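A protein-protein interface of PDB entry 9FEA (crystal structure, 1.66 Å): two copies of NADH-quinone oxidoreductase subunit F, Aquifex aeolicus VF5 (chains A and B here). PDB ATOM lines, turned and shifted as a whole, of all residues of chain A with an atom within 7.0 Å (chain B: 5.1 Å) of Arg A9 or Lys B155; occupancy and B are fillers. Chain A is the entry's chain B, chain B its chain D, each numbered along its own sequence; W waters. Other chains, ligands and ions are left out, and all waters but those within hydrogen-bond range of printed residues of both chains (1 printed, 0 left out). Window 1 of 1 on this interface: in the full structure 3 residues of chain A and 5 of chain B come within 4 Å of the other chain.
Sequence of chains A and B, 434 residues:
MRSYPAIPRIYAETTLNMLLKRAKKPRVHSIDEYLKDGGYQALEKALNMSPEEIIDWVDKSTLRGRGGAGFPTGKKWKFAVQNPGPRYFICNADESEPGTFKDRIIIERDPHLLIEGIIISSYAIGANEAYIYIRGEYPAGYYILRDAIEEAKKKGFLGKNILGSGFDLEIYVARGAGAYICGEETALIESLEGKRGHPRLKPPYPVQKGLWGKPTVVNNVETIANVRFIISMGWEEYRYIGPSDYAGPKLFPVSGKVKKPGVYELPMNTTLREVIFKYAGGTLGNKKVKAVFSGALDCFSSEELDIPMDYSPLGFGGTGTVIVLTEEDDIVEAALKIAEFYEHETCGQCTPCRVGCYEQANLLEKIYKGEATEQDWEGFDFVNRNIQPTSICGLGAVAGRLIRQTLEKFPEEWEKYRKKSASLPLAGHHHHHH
NE of Arg A9 lies within hydrogen-bond range of O of Lys B155.
The backbone carbonyl oxygen (O) of Ile A7 is in hydrogen-bond range of the guanidinium group (NH2) of Arg A9 (3.1 Å). The backbone carbonyl oxygen of Ala B152 is in hydrogen-bond range of the backbone NH of Phe B157, 2.9 Å away.
Among the printed residues, pairs that only touch across the chains: Arg A9 with Lys B154 (3.96 Å), Arg A9 with Phe B157 (3.9 Å), Arg A9 with Leu B163 (3.7 Å) and Tyr A11 with Lys B154 (3.6 Å).
Of the printed residues of chain B, Arg A9 touches Lys B154, Lys B155, Phe B157 and Leu B163. Ile A10 touches none of the printed residues of chain B. Printed residues of chain B within 4 Å of Tyr A11: Lys B154 (3.6 Å). Of the printed residues of chain A, Lys B154 touches Arg A9 (3.96 Å) and Tyr A11 (3.6 Å). Of chain A, only Arg A9 (3.0 Å) comes within 4 Å of Lys B155. Of the printed residues of chain A, Phe B157 touches Arg A9 (3.9 Å). Of the printed residues of chain A, Leu B163 touches Arg A9 (3.7 Å). The nearest residue of chain B that does not touch Arg A9 is Gly B156 (4.1 Å).
Of the 11 printed residues of chain A, 2 touch a printed residue of chain B. Of the 11 printed residues of chain B, 4 touch a printed residue of chain A. Hydrophobic or aromatic side chains of chain B that line the printed part of chain A: Phe B157 and Leu B163. Among the printed residues, 5 pairs touch across the chains. Among the printed residues, no Asp or Glu carboxylate lies within 4 Å of a Lys or Arg side-chain nitrogen of the other chain.
No position is printed for both chains. Of the 5 pairs that touch across the chains among the printed residues, none has its exchanged pair printed and touching as well.
Water W1 lies within hydrogen-bond range of the backbone carbonyl oxygen of Lys B154 (2.6 Å) and the backbone carbonyl oxygen of Ile A10 (3.1 Å).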
ATOM      1  N   ALA A   6       6.883 -29.808 -13.891  1.00  0.00           N
ATOM      2  CA  ALA A   6       6.176 -28.624 -13.418  1.00  0.00           C
ATOM      3  C   ALA A   6       4.736 -28.620 -13.940  1.00  0.00           C
ATOM      4  O   ALA A   6       4.498 -28.915 -15.109  1.00  0.00           O
ATOM      5  CB  ALA A   6       6.897 -27.373 -13.866  1.00  0.00           C
ATOM      6  N   ILE A   7       3.802 -28.278 -13.036  1.00  0.00           N
ATOM      7  CA  ILE A   7       2.395 -28.077 -13.346  1.00  0.00           C
ATOM      8  C   ILE A   7       2.006 -26.680 -12.874  1.00  0.00           C
ATOM      9  O   ILE A   7       2.411 -26.271 -11.783  1.00  0.00           O
ATOM     10  CB  ILE A   7       1.516 -29.122 -12.636  1.00  0.00           C
ATOM     11  CG1 ILE A   7       2.073 -30.540 -12.776  1.00  0.00           C
ATOM     12  CG2 ILE A   7       0.062 -29.017 -13.103  1.00  0.00           C
ATOM     13  CD1 ILE A   7       1.317 -31.574 -11.959  1.00  0.00           C
ATOM     14  N   PRO A   8       1.195 -25.905 -13.635  1.00  0.00           N
ATOM     15  CA  PRO A   8       0.672 -24.648 -13.103  1.00  0.00           C
ATOM     16  C   PRO A   8      -0.265 -24.984 -11.944  1.00  0.00           C
ATOM     17  O   PRO A   8      -0.876 -26.061 -11.929  1.00  0.00           O
ATOM     18  CB  PRO A   8      -0.061 -23.971 -14.257  1.00  0.00           C
ATOM     19  CG  PRO A   8       0.174 -24.852 -15.474  1.00  0.00           C
ATOM     20  CD  PRO A   8       0.766 -26.176 -15.015  1.00  0.00           C
ATOM     21  N   ARG A   9      -0.346 -24.068 -10.965  1.00  0.00           N
ATOM     22  CA  ARG A   9      -1.158 -24.307  -9.781  1.00  0.00           C
ATOM     23  C   ARG A   9      -2.557 -23.736 -10.014  1.00  0.00           C
ATOM     24  O   ARG A   9      -2.846 -22.582  -9.676  1.00  0.00           O
ATOM     25  CB  ARG A   9      -0.517 -23.719  -8.519  1.00  0.00           C
ATOM     26  CG  ARG A   9       0.564 -24.599  -7.887  1.00  0.00           C
ATOM     27  CD  ARG A   9       1.827 -24.710  -8.727  1.00  0.00           C
ATOM     28  NE  ARG A   9       2.489 -23.409  -8.818  1.00  0.00           N
ATOM     29  CZ  ARG A   9       3.540 -23.104  -9.580  1.00  0.00           C
ATOM     30  NH1 ARG A   9       4.075 -21.903  -9.490  1.00  0.00           N
ATOM     31  NH2 ARG A   9       4.061 -24.000 -10.391  1.00  0.00           N
ATOM     32  N   ILE A  10      -3.405 -24.545 -10.646  1.00  0.00           N
ATOM     33  CA  ILE A  10      -4.765 -24.141 -10.954  1.00  0.00           C
ATOM     34  C   ILE A  10      -5.516 -23.948  -9.638  1.00  0.00           C
ATOM     35  O   ILE A  10      -5.435 -24.814  -8.761  1.00  0.00           O
ATOM     36  CB  ILE A  10      -5.416 -25.203 -11.854  1.00  0.00           C
ATOM     37  CG1 ILE A  10      -4.719 -25.265 -13.203  1.00  0.00           C
ATOM     38  CG2 ILE A  10      -6.927 -24.980 -11.960  1.00  0.00           C
ATOM     39  CD1 ILE A  10      -5.051 -26.477 -14.049  1.00  0.00           C
ATOM     40  N   TYR A  11      -6.202 -22.815  -9.503  1.00  0.00           N
ATOM     41  CA  TYR A  11      -7.012 -22.550  -8.324  1.00  0.00           C
ATOM     42  C   TYR A  11      -8.201 -23.509  -8.278  1.00  0.00           C
ATOM     43  O   TYR A  11      -8.858 -23.755  -9.286  1.00  0.00           O
ATOM     44  CB  TYR A  11      -7.500 -21.105  -8.345  1.00  0.00           C
ATOM     45  CG  TYR A  11      -8.391 -20.807  -7.150  1.00  0.00           C
ATOM     46  CD1 TYR A  11      -7.871 -20.818  -5.860  1.00  0.00           C
ATOM     47  CD2 TYR A  11      -9.741 -20.524  -7.305  1.00  0.00           C
ATOM     48  CE1 TYR A  11      -8.678 -20.567  -4.762  1.00  0.00           C
ATOM     49  CE2 TYR A  11     -10.549 -20.234  -6.221  1.00  0.00           C
ATOM     50  CZ  TYR A  11     -10.016 -20.254  -4.938  1.00  0.00           C
ATOM     51  OH  TYR A  11     -10.821 -19.984  -3.858  1.00  0.00           O
ATOM     52  N   ALA A  12      -8.507 -24.030  -7.086  1.00  0.00           N
ATOM     53  CA  ALA A  12      -9.657 -24.904  -6.897  1.00  0.00           C
ATOM     54  C   ALA A  12     -10.354 -24.542  -5.587  1.00  0.00           C
ATOM     55  O   ALA A  12      -9.690 -24.189  -4.604  1.00  0.00           O
ATOM     56  CB  ALA A  12      -9.226 -26.346  -6.914  1.00  0.00           C
ATOM     57  N   PRO A  26      -2.957 -27.599  -4.160  1.00  0.00           N
ATOM     58  CA  PRO A  26      -2.282 -27.957  -5.410  1.00  0.00           C
ATOM     59  C   PRO A  26      -0.983 -28.716  -5.221  1.00  0.00           C
ATOM     60  O   PRO A  26       0.096 -28.172  -5.417  1.00  0.00           O
ATOM     61  CB  PRO A  26      -2.056 -26.571  -6.037  1.00  0.00           C
ATOM     62  CG  PRO A  26      -1.757 -25.699  -4.846  1.00  0.00           C
ATOM     63  CD  PRO A  26      -2.726 -26.196  -3.768  1.00  0.00           C
ATOM     64  N   ARG A  27      -1.107 -29.976  -4.824  1.00  0.00           N
ATOM     65  CA  ARG A  27       0.063 -30.812  -4.608  1.00  0.00           C
ATOM     66  C   ARG A  27      -0.397 -32.264  -4.637  1.00  0.00           C
ATOM     67  O   ARG A  27      -1.591 -32.532  -4.502  1.00  0.00           O
ATOM     68  CB  ARG A  27       0.744 -30.487  -3.275  1.00  0.00           C
ATOM     69  CG  ARG A  27      -0.115 -30.753  -2.050  1.00  0.00           C
ATOM     70  CD  ARG A  27       0.595 -30.406  -0.763  1.00  0.00           C
ATOM     71  NE  ARG A  27      -0.280 -30.636   0.393  1.00  0.00           N
ATOM     72  CZ  ARG A  27      -0.548 -31.843   0.916  1.00  0.00           C
ATOM     73  NH1 ARG A  27      -1.310 -31.957   1.981  1.00  0.00           N
ATOM     74  NH2 ARG A  27      -0.051 -32.940   0.379  1.00  0.00           N
ATOM     75  N   ARG A 109      -3.610 -34.399  -8.124  1.00  0.00           N
ATOM     76  CA  ARG A 109      -3.600 -34.005  -6.722  1.00  0.00           C
ATOM     77  C   ARG A 109      -4.127 -35.114  -5.811  1.00  0.00           C
ATOM     78  O   ARG A 109      -3.678 -35.224  -4.674  1.00  0.00           O
ATOM     79  CB  ARG A 109      -4.391 -32.722  -6.477  1.00  0.00           C
ATOM     80  CG  ARG A 109      -3.842 -31.578  -7.308  1.00  0.00           C
ATOM     81  CD  ARG A 109      -4.741 -30.371  -7.191  1.00  0.00           C
ATOM     82  NE  ARG A 109      -4.174 -29.304  -8.013  1.00  0.00           N
ATOM     83  CZ  ARG A 109      -4.634 -28.070  -8.032  1.00  0.00           C
ATOM     84  NH1 ARG A 109      -5.614 -27.713  -7.212  1.00  0.00           N
ATOM     85  NH2 ARG A 109      -4.065 -27.186  -8.823  1.00  0.00           N
ATOM     86  N   PRO A 261     -10.225 -17.476 -12.160  1.00  0.00           N
ATOM     87  CA  PRO A 261     -10.330 -18.672 -12.994  1.00  0.00           C
ATOM     88  C   PRO A 261      -9.817 -19.891 -12.214  1.00  0.00           C
ATOM     89  O   PRO A 261      -8.873 -19.782 -11.434  1.00  0.00           O
ATOM     90  CB  PRO A 261      -9.458 -18.319 -14.212  1.00  0.00           C
ATOM     91  CG  PRO A 261      -8.464 -17.334 -13.691  1.00  0.00           C
ATOM     92  CD  PRO A 261      -9.197 -16.533 -12.632  1.00  0.00           C
ATOM     93  N   ILE B  31      -0.506 -10.480  -6.203  1.00  0.00           N
ATOM     94  CA  ILE B  31       0.459 -11.479  -6.640  1.00  0.00           C
ATOM     95  C   ILE B  31       0.642 -11.474  -8.160  1.00  0.00           C
ATOM     96  O   ILE B  31       1.744 -11.699  -8.627  1.00  0.00           O
ATOM     97  CB  ILE B  31       0.084 -12.876  -6.113  1.00  0.00           C
ATOM     98  CG1 ILE B  31       1.270 -13.836  -6.156  1.00  0.00           C
ATOM     99  CG2 ILE B  31      -1.115 -13.446  -6.854  1.00  0.00           C
ATOM    100  CD1 ILE B  31       1.162 -14.962  -5.139  1.00  0.00           C
ATOM    101  N   ASP B  32      -0.411 -11.233  -8.944  1.00  0.00           N
ATOM    102  CA  ASP B  32      -0.267 -11.231 -10.395  1.00  0.00           C
ATOM    103  C   ASP B  32       0.732 -10.167 -10.840  1.00  0.00           C
ATOM    104  O   ASP B  32       1.590 -10.446 -11.676  1.00  0.00           O
ATOM    105  CB  ASP B  32      -1.596 -11.103 -11.115  1.00  0.00           C
ATOM    106  CG  ASP B  32      -2.369 -12.403 -11.264  1.00  0.00           C
ATOM    107  OD1 ASP B  32      -1.869 -13.467 -10.833  1.00  0.00           O
ATOM    108  OD2 ASP B  32      -3.451 -12.351 -11.868  1.00  0.00           O
ATOM    109  N   LEU B  35       4.171 -11.309  -9.853  1.00  0.00           N
ATOM    110  CA  LEU B  35       4.676 -12.369 -10.719  1.00  0.00           C
ATOM    111  C   LEU B  35       5.169 -11.803 -12.053  1.00  0.00           C
ATOM    112  O   LEU B  35       6.114 -12.334 -12.627  1.00  0.00           O
ATOM    113  CB  LEU B  35       3.616 -13.450 -10.947  1.00  0.00           C
ATOM    114  CG  LEU B  35       3.246 -14.295  -9.723  1.00  0.00           C
ATOM    115  CD1 LEU B  35       1.954 -15.032  -9.948  1.00  0.00           C
ATOM    116  CD2 LEU B  35       4.336 -15.262  -9.411  1.00  0.00           C
ATOM    117  N   GLU B 151      -2.954 -15.584  -1.125  1.00  0.00           N
ATOM    118  CA  GLU B 151      -2.578 -15.595  -2.531  1.00  0.00           C
ATOM    119  C   GLU B 151      -1.392 -16.532  -2.780  1.00  0.00           C
ATOM    120  O   GLU B 151      -1.409 -17.299  -3.749  1.00  0.00           O
ATOM    121  CB  GLU B 151      -2.167 -14.217  -3.065  1.00  0.00           C
ATOM    122  CG  GLU B 151      -3.294 -13.194  -3.150  1.00  0.00           C
ATOM    123  CD  GLU B 151      -2.827 -11.860  -3.742  1.00  0.00           C
ATOM    124  OE1 GLU B 151      -1.945 -11.177  -3.185  1.00  0.00           O
ATOM    125  OE2 GLU B 151      -3.313 -11.520  -4.843  1.00  0.00           O
ATOM    126  N   ALA B 152      -0.360 -16.438  -1.937  1.00  0.00           N
ATOM    127  CA  ALA B 152       0.829 -17.267  -2.069  1.00  0.00           C
ATOM    128  C   ALA B 152       0.460 -18.742  -1.900  1.00  0.00           C
ATOM    129  O   ALA B 152       0.932 -19.576  -2.653  1.00  0.00           O
ATOM    130  CB  ALA B 152       1.882 -16.832  -1.078  1.00  0.00           C
ATOM    131  N   LYS B 153      -0.414 -19.047  -0.935  1.00  0.00           N
ATOM    132  CA  LYS B 153      -0.885 -20.419  -0.773  1.00  0.00           C
ATOM    133  C   LYS B 153      -1.531 -20.911  -2.062  1.00  0.00           C
ATOM    134  O   LYS B 153      -1.210 -21.990  -2.559  1.00  0.00           O
ATOM    135  CB  LYS B 153      -1.915 -20.530   0.357  1.00  0.00           C
ATOM    136  CG  LYS B 153      -1.391 -20.490   1.776  1.00  0.00           C
ATOM    137  CD  LYS B 153      -2.574 -20.535   2.744  1.00  0.00           C
ATOM    138  CE  LYS B 153      -2.326 -21.150   4.075  1.00  0.00           C
ATOM    139  NZ  LYS B 153      -2.479 -22.609   4.048  1.00  0.00           N
ATOM    140  N   LYS B 154      -2.427 -20.087  -2.628  1.00  0.00           N
ATOM    141  CA  LYS B 154      -3.188 -20.481  -3.802  1.00  0.00           C
ATOM    142  C   LYS B 154      -2.258 -20.815  -4.973  1.00  0.00           C
ATOM    143  O   LYS B 154      -2.540 -21.720  -5.763  1.00  0.00           O
ATOM    144  CB  LYS B 154      -4.239 -19.405  -4.107  1.00  0.00           C
ATOM    145  CG  LYS B 154      -5.331 -19.359  -3.019  1.00  0.00           C
ATOM    146  CD  LYS B 154      -6.414 -18.294  -3.170  1.00  0.00           C
ATOM    147  CE  LYS B 154      -7.268 -18.204  -1.930  1.00  0.00           C
ATOM    148  NZ  LYS B 154      -8.497 -17.449  -2.192  1.00  0.00           N
ATOM    149  N   LYS B 155      -1.144 -20.086  -5.073  1.00  0.00           N
ATOM    150  CA  LYS B 155      -0.189 -20.277  -6.144  1.00  0.00           C
ATOM    151  C   LYS B 155       0.846 -21.332  -5.790  1.00  0.00           C
ATOM    152  O   LYS B 155       1.744 -21.573  -6.583  1.00  0.00           O
ATOM    153  CB  LYS B 155       0.519 -18.956  -6.483  1.00  0.00           C
ATOM    154  CG  LYS B 155      -0.363 -17.909  -7.143  1.00  0.00           C
ATOM    155  CD  LYS B 155      -0.749 -18.290  -8.557  1.00  0.00           C
ATOM    156  CE  LYS B 155      -1.313 -17.184  -9.391  1.00  0.00           C
ATOM    157  NZ  LYS B 155      -1.590 -17.706 -10.742  1.00  0.00           N
ATOM    158  N   GLY B 156       0.731 -21.945  -4.604  1.00  0.00           N
ATOM    159  CA  GLY B 156       1.572 -23.071  -4.242  1.00  0.00           C
ATOM    160  C   GLY B 156       2.939 -22.676  -3.696  1.00  0.00           C
ATOM    161  O   GLY B 156       3.833 -23.521  -3.652  1.00  0.00           O
ATOM    162  N   PHE B 157       3.076 -21.439  -3.187  1.00  0.00           N
ATOM    163  CA  PHE B 157       4.341 -20.989  -2.612  1.00  0.00           C
ATOM    164  C   PHE B 157       4.393 -21.210  -1.099  1.00  0.00           C
ATOM    165  O   PHE B 157       5.446 -21.024  -0.480  1.00  0.00           O
ATOM    166  CB  PHE B 157       4.566 -19.514  -2.958  1.00  0.00           C
ATOM    167  CG  PHE B 157       4.628 -19.215  -4.447  1.00  0.00           C
ATOM    168  CD1 PHE B 157       5.501 -19.904  -5.284  1.00  0.00           C
ATOM    169  CD2 PHE B 157       3.792 -18.265  -5.017  1.00  0.00           C
ATOM    170  CE1 PHE B 157       5.547 -19.641  -6.646  1.00  0.00           C
ATOM    171  CE2 PHE B 157       3.829 -18.012  -6.386  1.00  0.00           C
ATOM    172  CZ  PHE B 157       4.716 -18.693  -7.195  1.00  0.00           C
ATOM    173  N   LEU B 163       6.232 -26.573  -4.176  1.00  0.00           N
ATOM    174  CA  LEU B 163       6.771 -26.765  -5.520  1.00  0.00           C
ATOM    175  C   LEU B 163       7.576 -28.061  -5.613  1.00  0.00           C
ATOM    176  O   LEU B 163       8.557 -28.137  -6.354  1.00  0.00           O
ATOM    177  CB  LEU B 163       7.603 -25.552  -5.929  1.00  0.00           C
ATOM    178  CG  LEU B 163       6.901 -24.192  -5.830  1.00  0.00           C
ATOM    179  CD1 LEU B 163       7.883 -23.075  -6.143  1.00  0.00           C
ATOM    180  CD2 LEU B 163       5.703 -24.117  -6.763  1.00  0.00           C
HETATM  181  O   HOH W   1      -4.090 -23.743  -6.232  1.00  0.00           O
